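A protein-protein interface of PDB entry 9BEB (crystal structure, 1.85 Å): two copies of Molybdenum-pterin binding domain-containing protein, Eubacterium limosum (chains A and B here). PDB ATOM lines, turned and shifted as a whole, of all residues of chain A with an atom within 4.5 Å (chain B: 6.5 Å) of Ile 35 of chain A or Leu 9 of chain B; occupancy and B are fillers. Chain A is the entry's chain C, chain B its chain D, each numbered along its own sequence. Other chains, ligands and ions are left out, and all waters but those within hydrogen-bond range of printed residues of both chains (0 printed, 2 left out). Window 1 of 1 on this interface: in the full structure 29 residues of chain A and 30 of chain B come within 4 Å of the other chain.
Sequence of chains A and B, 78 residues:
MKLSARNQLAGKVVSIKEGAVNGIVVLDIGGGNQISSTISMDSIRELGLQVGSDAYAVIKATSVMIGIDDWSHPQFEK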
ATOM      1  N   VAL A  25       7.200  19.782 -13.124  1.00  0.00           N
ATOM      2  CA  VAL A  25       6.882  20.800 -12.140  1.00  0.00           C
ATOM      3  C   VAL A  25       7.611  20.441 -10.860  1.00  0.00           C
ATOM      4  O   VAL A  25       7.515  19.306 -10.368  1.00  0.00           O
ATOM      5  CB  VAL A  25       5.368  20.877 -11.886  1.00  0.00           C
ATOM      6  CG1 VAL A  25       5.069  21.911 -10.801  1.00  0.00           C
ATOM      7  CG2 VAL A  25       4.624  21.199 -13.169  1.00  0.00           C
ATOM      8  N   VAL A  26       8.302  21.412 -10.280  1.00  0.00           N
ATOM      9  CA  VAL A  26       8.957  21.226  -8.990  1.00  0.00           C
ATOM     10  C   VAL A  26       8.215  22.047  -7.954  1.00  0.00           C
ATOM     11  O   VAL A  26       8.014  23.258  -8.139  1.00  0.00           O
ATOM     12  CB  VAL A  26      10.435  21.639  -9.029  1.00  0.00           C
ATOM     13  CG1 VAL A  26      11.050  21.558  -7.640  1.00  0.00           C
ATOM     14  CG2 VAL A  26      11.208  20.795 -10.074  1.00  0.00           C
ATOM     15  N   LEU A  27       7.818  21.383  -6.865  1.00  0.00           N
ATOM     16  CA  LEU A  27       7.122  22.019  -5.755  1.00  0.00           C
ATOM     17  C   LEU A  27       7.978  22.006  -4.495  1.00  0.00           C
ATOM     18  O   LEU A  27       8.499  20.960  -4.110  1.00  0.00           O
ATOM     19  CB  LEU A  27       5.819  21.280  -5.454  1.00  0.00           C
ATOM     20  CG  LEU A  27       4.454  21.535  -6.059  1.00  0.00           C
ATOM     21  CD1 LEU A  27       3.471  20.653  -5.177  1.00  0.00           C
ATOM     22  CD2 LEU A  27       4.028  22.953  -6.046  1.00  0.00           C
ATOM     23  N   ILE A  29       7.635  21.820  -0.804  1.00  0.00           N
ATOM     24  CA  ILE A  29       6.610  21.406   0.154  1.00  0.00           C
ATOM     25  C   ILE A  29       7.027  21.709   1.586  1.00  0.00           C
ATOM     26  O   ILE A  29       6.366  21.271   2.525  1.00  0.00           O
ATOM     27  CB  ILE A  29       6.250  19.915   0.001  1.00  0.00           C
ATOM     28  CG1 ILE A  29       7.436  19.014   0.364  1.00  0.00           C
ATOM     29  CG2 ILE A  29       5.751  19.641  -1.403  1.00  0.00           C
ATOM     30  CD1 ILE A  29       7.025  17.574   0.600  1.00  0.00           C
ATOM     31  N   ASN A  33      12.236  20.074   1.711  1.00  0.00           N
ATOM     32  CA  ASN A  33      11.938  19.089   0.682  1.00  0.00           C
ATOM     33  C   ASN A  33      11.280  19.705  -0.541  1.00  0.00           C
ATOM     34  O   ASN A  33      10.484  20.644  -0.440  1.00  0.00           O
ATOM     35  CB  ASN A  33      11.030  17.997   1.227  1.00  0.00           C
ATOM     36  CG  ASN A  33      11.717  17.149   2.273  1.00  0.00           C
ATOM     37  OD1 ASN A  33      12.869  16.751   2.095  1.00  0.00           O
ATOM     38  ND2 ASN A  33      11.031  16.893   3.365  1.00  0.00           N
ATOM     39  N   GLN A  34      11.598  19.124  -1.707  1.00  0.00           N
ATOM     40  CA  GLN A  34      10.984  19.449  -2.990  1.00  0.00           C
ATOM     41  C   GLN A  34      10.491  18.164  -3.648  1.00  0.00           C
ATOM     42  O   GLN A  34      11.008  17.076  -3.383  1.00  0.00           O
ATOM     43  CB  GLN A  34      11.979  20.186  -3.890  1.00  0.00           C
ATOM     44  CG  GLN A  34      12.515  21.453  -3.213  1.00  0.00           C
ATOM     45  CD  GLN A  34      13.255  22.375  -4.150  1.00  0.00           C
ATOM     46  OE1 GLN A  34      13.810  21.946  -5.165  1.00  0.00           O
ATOM     47  NE2 GLN A  34      13.282  23.663  -3.797  1.00  0.00           N
ATOM     48  N   ILE A  35       9.439  18.286  -4.443  1.00  0.00           N
ATOM     49  CA  ILE A  35       8.860  17.161  -5.181  1.00  0.00           C
ATOM     50  C   ILE A  35       8.803  17.533  -6.644  1.00  0.00           C
ATOM     51  O   ILE A  35       8.340  18.629  -6.978  1.00  0.00           O
ATOM     52  CB  ILE A  35       7.444  16.822  -4.675  1.00  0.00           C
ATOM     53  CG1 ILE A  35       7.494  16.483  -3.192  1.00  0.00           C
ATOM     54  CG2 ILE A  35       6.865  15.685  -5.485  1.00  0.00           C
ATOM     55  CD1 ILE A  35       7.733  15.063  -2.935  1.00  0.00           C
ATOM     56  N   SER A  36       9.287  16.632  -7.500  1.00  0.00           N
ATOM     57  CA  SER A  36       9.231  16.795  -8.943  1.00  0.00           C
ATOM     58  C   SER A  36       8.109  15.928  -9.495  1.00  0.00           C
ATOM     59  O   SER A  36       7.983  14.750  -9.122  1.00  0.00           O
ATOM     60  CB  SER A  36      10.557  16.409  -9.595  1.00  0.00           C
ATOM     61  OG  SER A  36      11.562  17.288  -9.174  1.00  0.00           O
ATOM     62  N   SER A  37       7.314  16.511 -10.395  1.00  0.00           N
ATOM     63  CA  SER A  37       6.143  15.876 -10.986  1.00  0.00           C
ATOM     64  C   SER A  37       6.247  15.956 -12.507  1.00  0.00           C
ATOM     65  O   SER A  37       6.376  17.046 -13.071  1.00  0.00           O
ATOM     66  CB  SER A  37       4.864  16.560 -10.503  1.00  0.00           C
ATOM     67  OG  SER A  37       3.762  16.206 -11.277  1.00  0.00           O
ATOM     68  N   ALA A  57       1.321  18.281  -4.357  1.00  0.00           N
ATOM     69  CA  ALA A  57       1.861  17.066  -4.949  1.00  0.00           C
ATOM     70  C   ALA A  57       0.995  15.882  -4.531  1.00  0.00           C
ATOM     71  O   ALA A  57       0.877  15.596  -3.345  1.00  0.00           O
ATOM     72  CB  ALA A  57       3.305  16.833  -4.525  1.00  0.00           C
ATOM     73  N   ARG B   6      13.225  10.998  -9.059  1.00  0.00           N
ATOM     74  CA  ARG B   6      13.547  12.372  -8.713  1.00  0.00           C
ATOM     75  C   ARG B   6      13.256  12.682  -7.254  1.00  0.00           C
ATOM     76  O   ARG B   6      13.786  13.663  -6.715  1.00  0.00           O
ATOM     77  CB  ARG B   6      12.751  13.372  -9.547  1.00  0.00           C
ATOM     78  CG  ARG B   6      12.859  13.239 -11.027  1.00  0.00           C
ATOM     79  CD  ARG B   6      14.078  13.851 -11.527  1.00  0.00           C
ATOM     80  NE  ARG B   6      15.218  12.980 -11.276  1.00  0.00           N
ATOM     81  CZ  ARG B   6      16.467  13.414 -11.144  1.00  0.00           C
ATOM     82  NH1 ARG B   6      16.732  14.709 -11.252  1.00  0.00           N
ATOM     83  NH2 ARG B   6      17.443  12.556 -10.896  1.00  0.00           N
ATOM     84  N   ASN B   7      12.434  11.880  -6.591  1.00  0.00           N
ATOM     85  CA  ASN B   7      11.994  12.188  -5.230  1.00  0.00           C
ATOM     86  C   ASN B   7      12.515  11.138  -4.266  1.00  0.00           C
ATOM     87  O   ASN B   7      12.134   9.974  -4.340  1.00  0.00           O
ATOM     88  CB  ASN B   7      10.475  12.285  -5.195  1.00  0.00           C
ATOM     89  CG  ASN B   7       9.940  13.218  -6.266  1.00  0.00           C
ATOM     90  OD1 ASN B   7      10.208  14.412  -6.235  1.00  0.00           O
ATOM     91  ND2 ASN B   7       9.203  12.677  -7.222  1.00  0.00           N
ATOM     92  N   GLN B   8      13.367  11.563  -3.335  1.00  0.00           N
ATOM     93  CA  GLN B   8      13.963  10.650  -2.343  1.00  0.00           C
ATOM     94  C   GLN B   8      13.990  11.435  -1.033  1.00  0.00           C
ATOM     95  O   GLN B   8      14.927  12.183  -0.762  1.00  0.00           O
ATOM     96  CB  GLN B   8      15.338  10.180  -2.795  1.00  0.00           C
ATOM     97  CG  GLN B   8      15.302   9.434  -4.118  1.00  0.00           C
ATOM     98  CD  GLN B   8      16.656   9.088  -4.661  1.00  0.00           C
ATOM     99  OE1 GLN B   8      17.607   8.929  -3.901  1.00  0.00           O
ATOM    100  NE2 GLN B   8      16.760   8.966  -6.009  1.00  0.00           N
ATOM    101  N   LEU B   9      12.956  11.252  -0.222  1.00  0.00           N
ATOM    102  CA  LEU B   9      12.676  12.117   0.915  1.00  0.00           C
ATOM    103  C   LEU B   9      12.960  11.384   2.219  1.00  0.00           C
ATOM    104  O   LEU B   9      12.277  10.415   2.572  1.00  0.00           O
ATOM    105  CB  LEU B   9      11.224  12.601   0.859  1.00  0.00           C
ATOM    106  CG  LEU B   9      10.860  13.164  -0.515  1.00  0.00           C
ATOM    107  CD1 LEU B   9       9.380  13.309  -0.719  1.00  0.00           C
ATOM    108  CD2 LEU B   9      11.546  14.511  -0.685  1.00  0.00           C
ATOM    109  N   ALA B  10      13.963  11.871   2.941  1.00  0.00           N
ATOM    110  CA  ALA B  10      14.335  11.259   4.198  1.00  0.00           C
ATOM    111  C   ALA B  10      13.237  11.477   5.231  1.00  0.00           C
ATOM    112  O   ALA B  10      12.599  12.520   5.275  1.00  0.00           O
ATOM    113  CB  ALA B  10      15.668  11.825   4.685  1.00  0.00           C
ATOM    114  N   GLY B  11      13.039  10.479   6.076  1.00  0.00           N
ATOM    115  CA  GLY B  11      12.058  10.597   7.138  1.00  0.00           C
ATOM    116  C   GLY B  11      12.160   9.434   8.096  1.00  0.00           C
ATOM    117  O   GLY B  11      12.928   8.496   7.887  1.00  0.00           O
ATOM    118  N   LEU B  27       5.852   7.624   6.861  1.00  0.00           N
ATOM    119  CA  LEU B  27       7.099   8.296   7.165  1.00  0.00           C
ATOM    120  C   LEU B  27       6.839   9.763   7.489  1.00  0.00           C
ATOM    121  O   LEU B  27       6.102  10.433   6.755  1.00  0.00           O
ATOM    122  CB  LEU B  27       8.040   8.213   5.968  1.00  0.00           C
ATOM    123  CG  LEU B  27       8.808   6.960   5.622  1.00  0.00           C
ATOM    124  CD1 LEU B  27       9.886   7.421   4.559  1.00  0.00           C
ATOM    125  CD2 LEU B  27       9.427   6.375   6.840  1.00  0.00           C
ATOM    126  N   ILE B  29       8.434  13.147   7.128  1.00  0.00           N
ATOM    127  CA  ILE B  29       9.493  13.727   6.299  1.00  0.00           C
ATOM    128  C   ILE B  29       9.801  15.174   6.678  1.00  0.00           C
ATOM    129  O   ILE B  29      10.532  15.854   5.950  1.00  0.00           O
ATOM    130  CB  ILE B  29       9.167  13.631   4.801  1.00  0.00           C
ATOM    131  CG1 ILE B  29       7.911  14.429   4.446  1.00  0.00           C
ATOM    132  CG2 ILE B  29       9.017  12.150   4.356  1.00  0.00           C
ATOM    133  CD1 ILE B  29       7.813  14.683   2.964  1.00  0.00           C
ATOM    134  N   ILE B  35       4.309  10.837   4.534  1.00  0.00           N
ATOM    135  CA  ILE B  35       4.095  10.120   3.287  1.00  0.00           C
ATOM    136  C   ILE B  35       3.745   8.683   3.617  1.00  0.00           C
ATOM    137  O   ILE B  35       4.416   8.051   4.443  1.00  0.00           O
ATOM    138  CB  ILE B  35       5.320  10.201   2.355  1.00  0.00           C
ATOM    139  CG1 ILE B  35       5.418  11.609   1.783  1.00  0.00           C
ATOM    140  CG2 ILE B  35       5.160   9.231   1.215  1.00  0.00           C
ATOM    141  CD1 ILE B  35       6.466  11.818   0.738  1.00  0.00           C
ATOM    142  N   ALA B  55      14.472   6.214   7.210  1.00  0.00           N
ATOM    143  CA  ALA B  55      14.219   5.678   5.879  1.00  0.00           C
ATOM    144  C   ALA B  55      14.039   6.833   4.910  1.00  0.00           C
ATOM    145  O   ALA B  55      14.172   8.005   5.276  1.00  0.00           O
ATOM    146  CB  ALA B  55      12.987   4.768   5.870  1.00  0.00           C
ATOM    147  N   TYR B  56      13.668   6.489   3.683  1.00  0.00           N
ATOM    148  CA  TYR B  56      13.394   7.440   2.628  1.00  0.00           C
ATOM    149  C   TYR B  56      12.116   7.023   1.905  1.00  0.00           C
ATOM    150  O   TYR B  56      11.904   5.833   1.648  1.00  0.00           O
ATOM    151  CB  TYR B  56      14.509   7.495   1.559  1.00  0.00           C
ATOM    152  CG  TYR B  56      15.888   7.831   2.046  1.00  0.00           C
ATOM    153  CD1 TYR B  56      16.689   6.859   2.618  1.00  0.00           C
ATOM    154  CD2 TYR B  56      16.397   9.108   1.913  1.00  0.00           C
ATOM    155  CE1 TYR B  56      17.961   7.155   3.083  1.00  0.00           C
ATOM    156  CE2 TYR B  56      17.663   9.415   2.366  1.00  0.00           C
ATOM    157  CZ  TYR B  56      18.443   8.435   2.947  1.00  0.00           C
ATOM    158  OH  TYR B  56      19.712   8.748   3.387  1.00  0.00           O
ATOM    159  N   ALA B  57      11.304   8.013   1.541  1.00  0.00           N
ATOM    160  CA  ALA B  57      10.197   7.840   0.598  1.00  0.00           C
ATOM    161  C   ALA B  57      10.691   8.124  -0.821  1.00  0.00           C
ATOM    162  O   ALA B  57      11.176   9.222  -1.105  1.00  0.00           O
ATOM    163  CB  ALA B  57       9.032   8.762   0.941  1.00  0.00           C
ATOM    164  N   VAL B  58      10.546   7.144  -1.695  1.00  0.00           N
ATOM    165  CA  VAL B  58      11.113   7.182  -3.047  1.00  0.00           C
ATOM    166  C   VAL B  58       9.974   7.128  -4.057  1.00  0.00           C
ATOM    167  O   VAL B  58       9.187   6.173  -4.053  1.00  0.00           O
ATOM    168  CB  VAL B  58      12.100   6.033  -3.271  1.00  0.00           C
ATOM    169  CG1 VAL B  58      12.639   6.055  -4.692  1.00  0.00           C
ATOM    170  CG2 VAL B  58      13.259   6.106  -2.231  1.00  0.00           C
ATOM    171  N   ILE B  59       9.892   8.148  -4.921  1.00  0.00           N
ATOM    172  CA  ILE B  59       8.769   8.288  -5.853  1.00  0.00           C
ATOM    173  C   ILE B  59       9.302   8.760  -7.198  1.00  0.00           C
ATOM    174  O   ILE B  59       9.941   9.819  -7.292  1.00  0.00           O
ATOM    175  CB  ILE B  59       7.699   9.258  -5.360  1.00  0.00           C
ATOM    176  CG1 ILE B  59       7.352   8.918  -3.896  1.00  0.00           C
ATOM    177  CG2 ILE B  59       6.452   9.106  -6.264  1.00  0.00           C
ATOM    178  CD1 ILE B  59       7.379  10.112  -2.987  1.00  0.00           C
ATOM    179  N   VAL B  64       3.806  11.288  -9.862  1.00  0.00           N
ATOM    180  CA  VAL B  64       3.368  12.439  -9.080  1.00  0.00           C
ATOM    181  C   VAL B  64       2.453  13.287  -9.952  1.00  0.00           C
ATOM    182  O   VAL B  64       2.857  13.754 -11.023  1.00  0.00           O
ATOM    183  CB  VAL B  64       4.576  13.268  -8.603  1.00  0.00           C
ATOM    184  CG1 VAL B  64       4.111  14.488  -7.831  1.00  0.00           C
ATOM    185  CG2 VAL B  64       5.533  12.421  -7.763  1.00  0.00           C
ATOM    186  N   ILE B  66      -0.156  16.818 -10.032  1.00  0.00           N
ATOM    187  CA  ILE B  66      -0.284  18.130  -9.418  1.00  0.00           C
ATOM    188  C   ILE B  66      -1.757  18.466  -9.233  1.00  0.00           C
ATOM    189  O   ILE B  66      -2.553  18.306 -10.162  1.00  0.00           O
ATOM    190  CB  ILE B  66       0.395  19.229 -10.246  1.00  0.00           C
ATOM    191  CG1 ILE B  66       1.898  18.978 -10.392  1.00  0.00           C
ATOM    192  CG2 ILE B  66       0.171  20.599  -9.550  1.00  0.00           C
ATOM    193  CD1 ILE B  66       2.621  19.075  -9.075  1.00  0.00           C
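N of Ser 36 of chain A sits at hydrogen-bond distance from OD1 of Asn 7 of chain B, at 2.7 Å.
The backbone carbonyl oxygen (O) of Val 64 of chain B is in hydrogen-bond range of the side-chain hydroxyl (OG) of Ser 37 of chain A, 2.6 Å away.
ND2 of Asn 33 of chain A lies within hydrogen-bond range of O of Ile 29 of chain B (2.8 Å).
The backbone carbonyl oxygen (O) of Asn 7 of chain B sits at hydrogen-bond distance from the backbone NH (N) of Ile 59 of chain B (2.9 Å).
N of Ser 37 of chain A lies within hydrogen-bond range of O of Val 25 of chain A.
N of Ala 57 of chain B lies within hydrogen-bond range of O of Leu 9 of chain B.
The backbone NH of Leu 27 of chain A is in hydrogen-bond range of the backbone carbonyl oxygen of Ile 35 of chain A (2.8 Å).
Ile 29 of chain A touches Ile 29 of chain B (CD1 to CD1, 3.8 Å).
Leu 9 of chain B touches Asn 33 of chain A (CD2 to OD1, 3.8 Å).
Gln 34 of chain A touches Asn 7 of chain B.
CD2 of Leu 9 of chain B touches O of Gln 34 of chain A, 3.8 Å away.
Ile 35 of chain A touches Asn 7 of chain B.
Ile 35 of chain A touches Leu 9 of chain B (CD1 to CD1, 3.3 Å).
CG1 of Val 64 of chain B touches CG2 of Ile 35 of chain A (3.8 Å).
Arg 6 of chain B touches Ser 36 of chain A.
Val 64 of chain B touches Ser 36 of chain A.
Ser 37 of chain A touches Ile 66 of chain B (OG to CG1, 3.5 Å).
Ile 35 of chain A touches three residues of chain B.
Of the printed residues of chain A, Arg 6 of chain B touches Ser 36.
Of chain A, only Asn 33, Gln 34 and Ile 35 come within 4 Å of Leu 9 of chain B.
Ile 59 of chain B touches none of the printed residues of chain A.
Printed residues of chain A within 4 Å of Val 64 of chain B: Ile 35 (3.8 Å), Ser 36 (3.6 Å) and Ser 37 (2.6 Å).
Printed residues of chain A within 4 Å of Ile 66 of chain B: Ser 37.
The nearest residue of chain B that does not touch Ile 35 of chain A is Ile 59 of chain B (5.0 Å).
Hydrophobic or aromatic side chains of chain A that line the printed part of chain B: Ile 29 and Ile 35.
Of the 16 printed residues of chain B, 6 touch a printed residue of chain A.
Ile 29 of chain B touches its own counterpart, Ile 29 of chain A.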
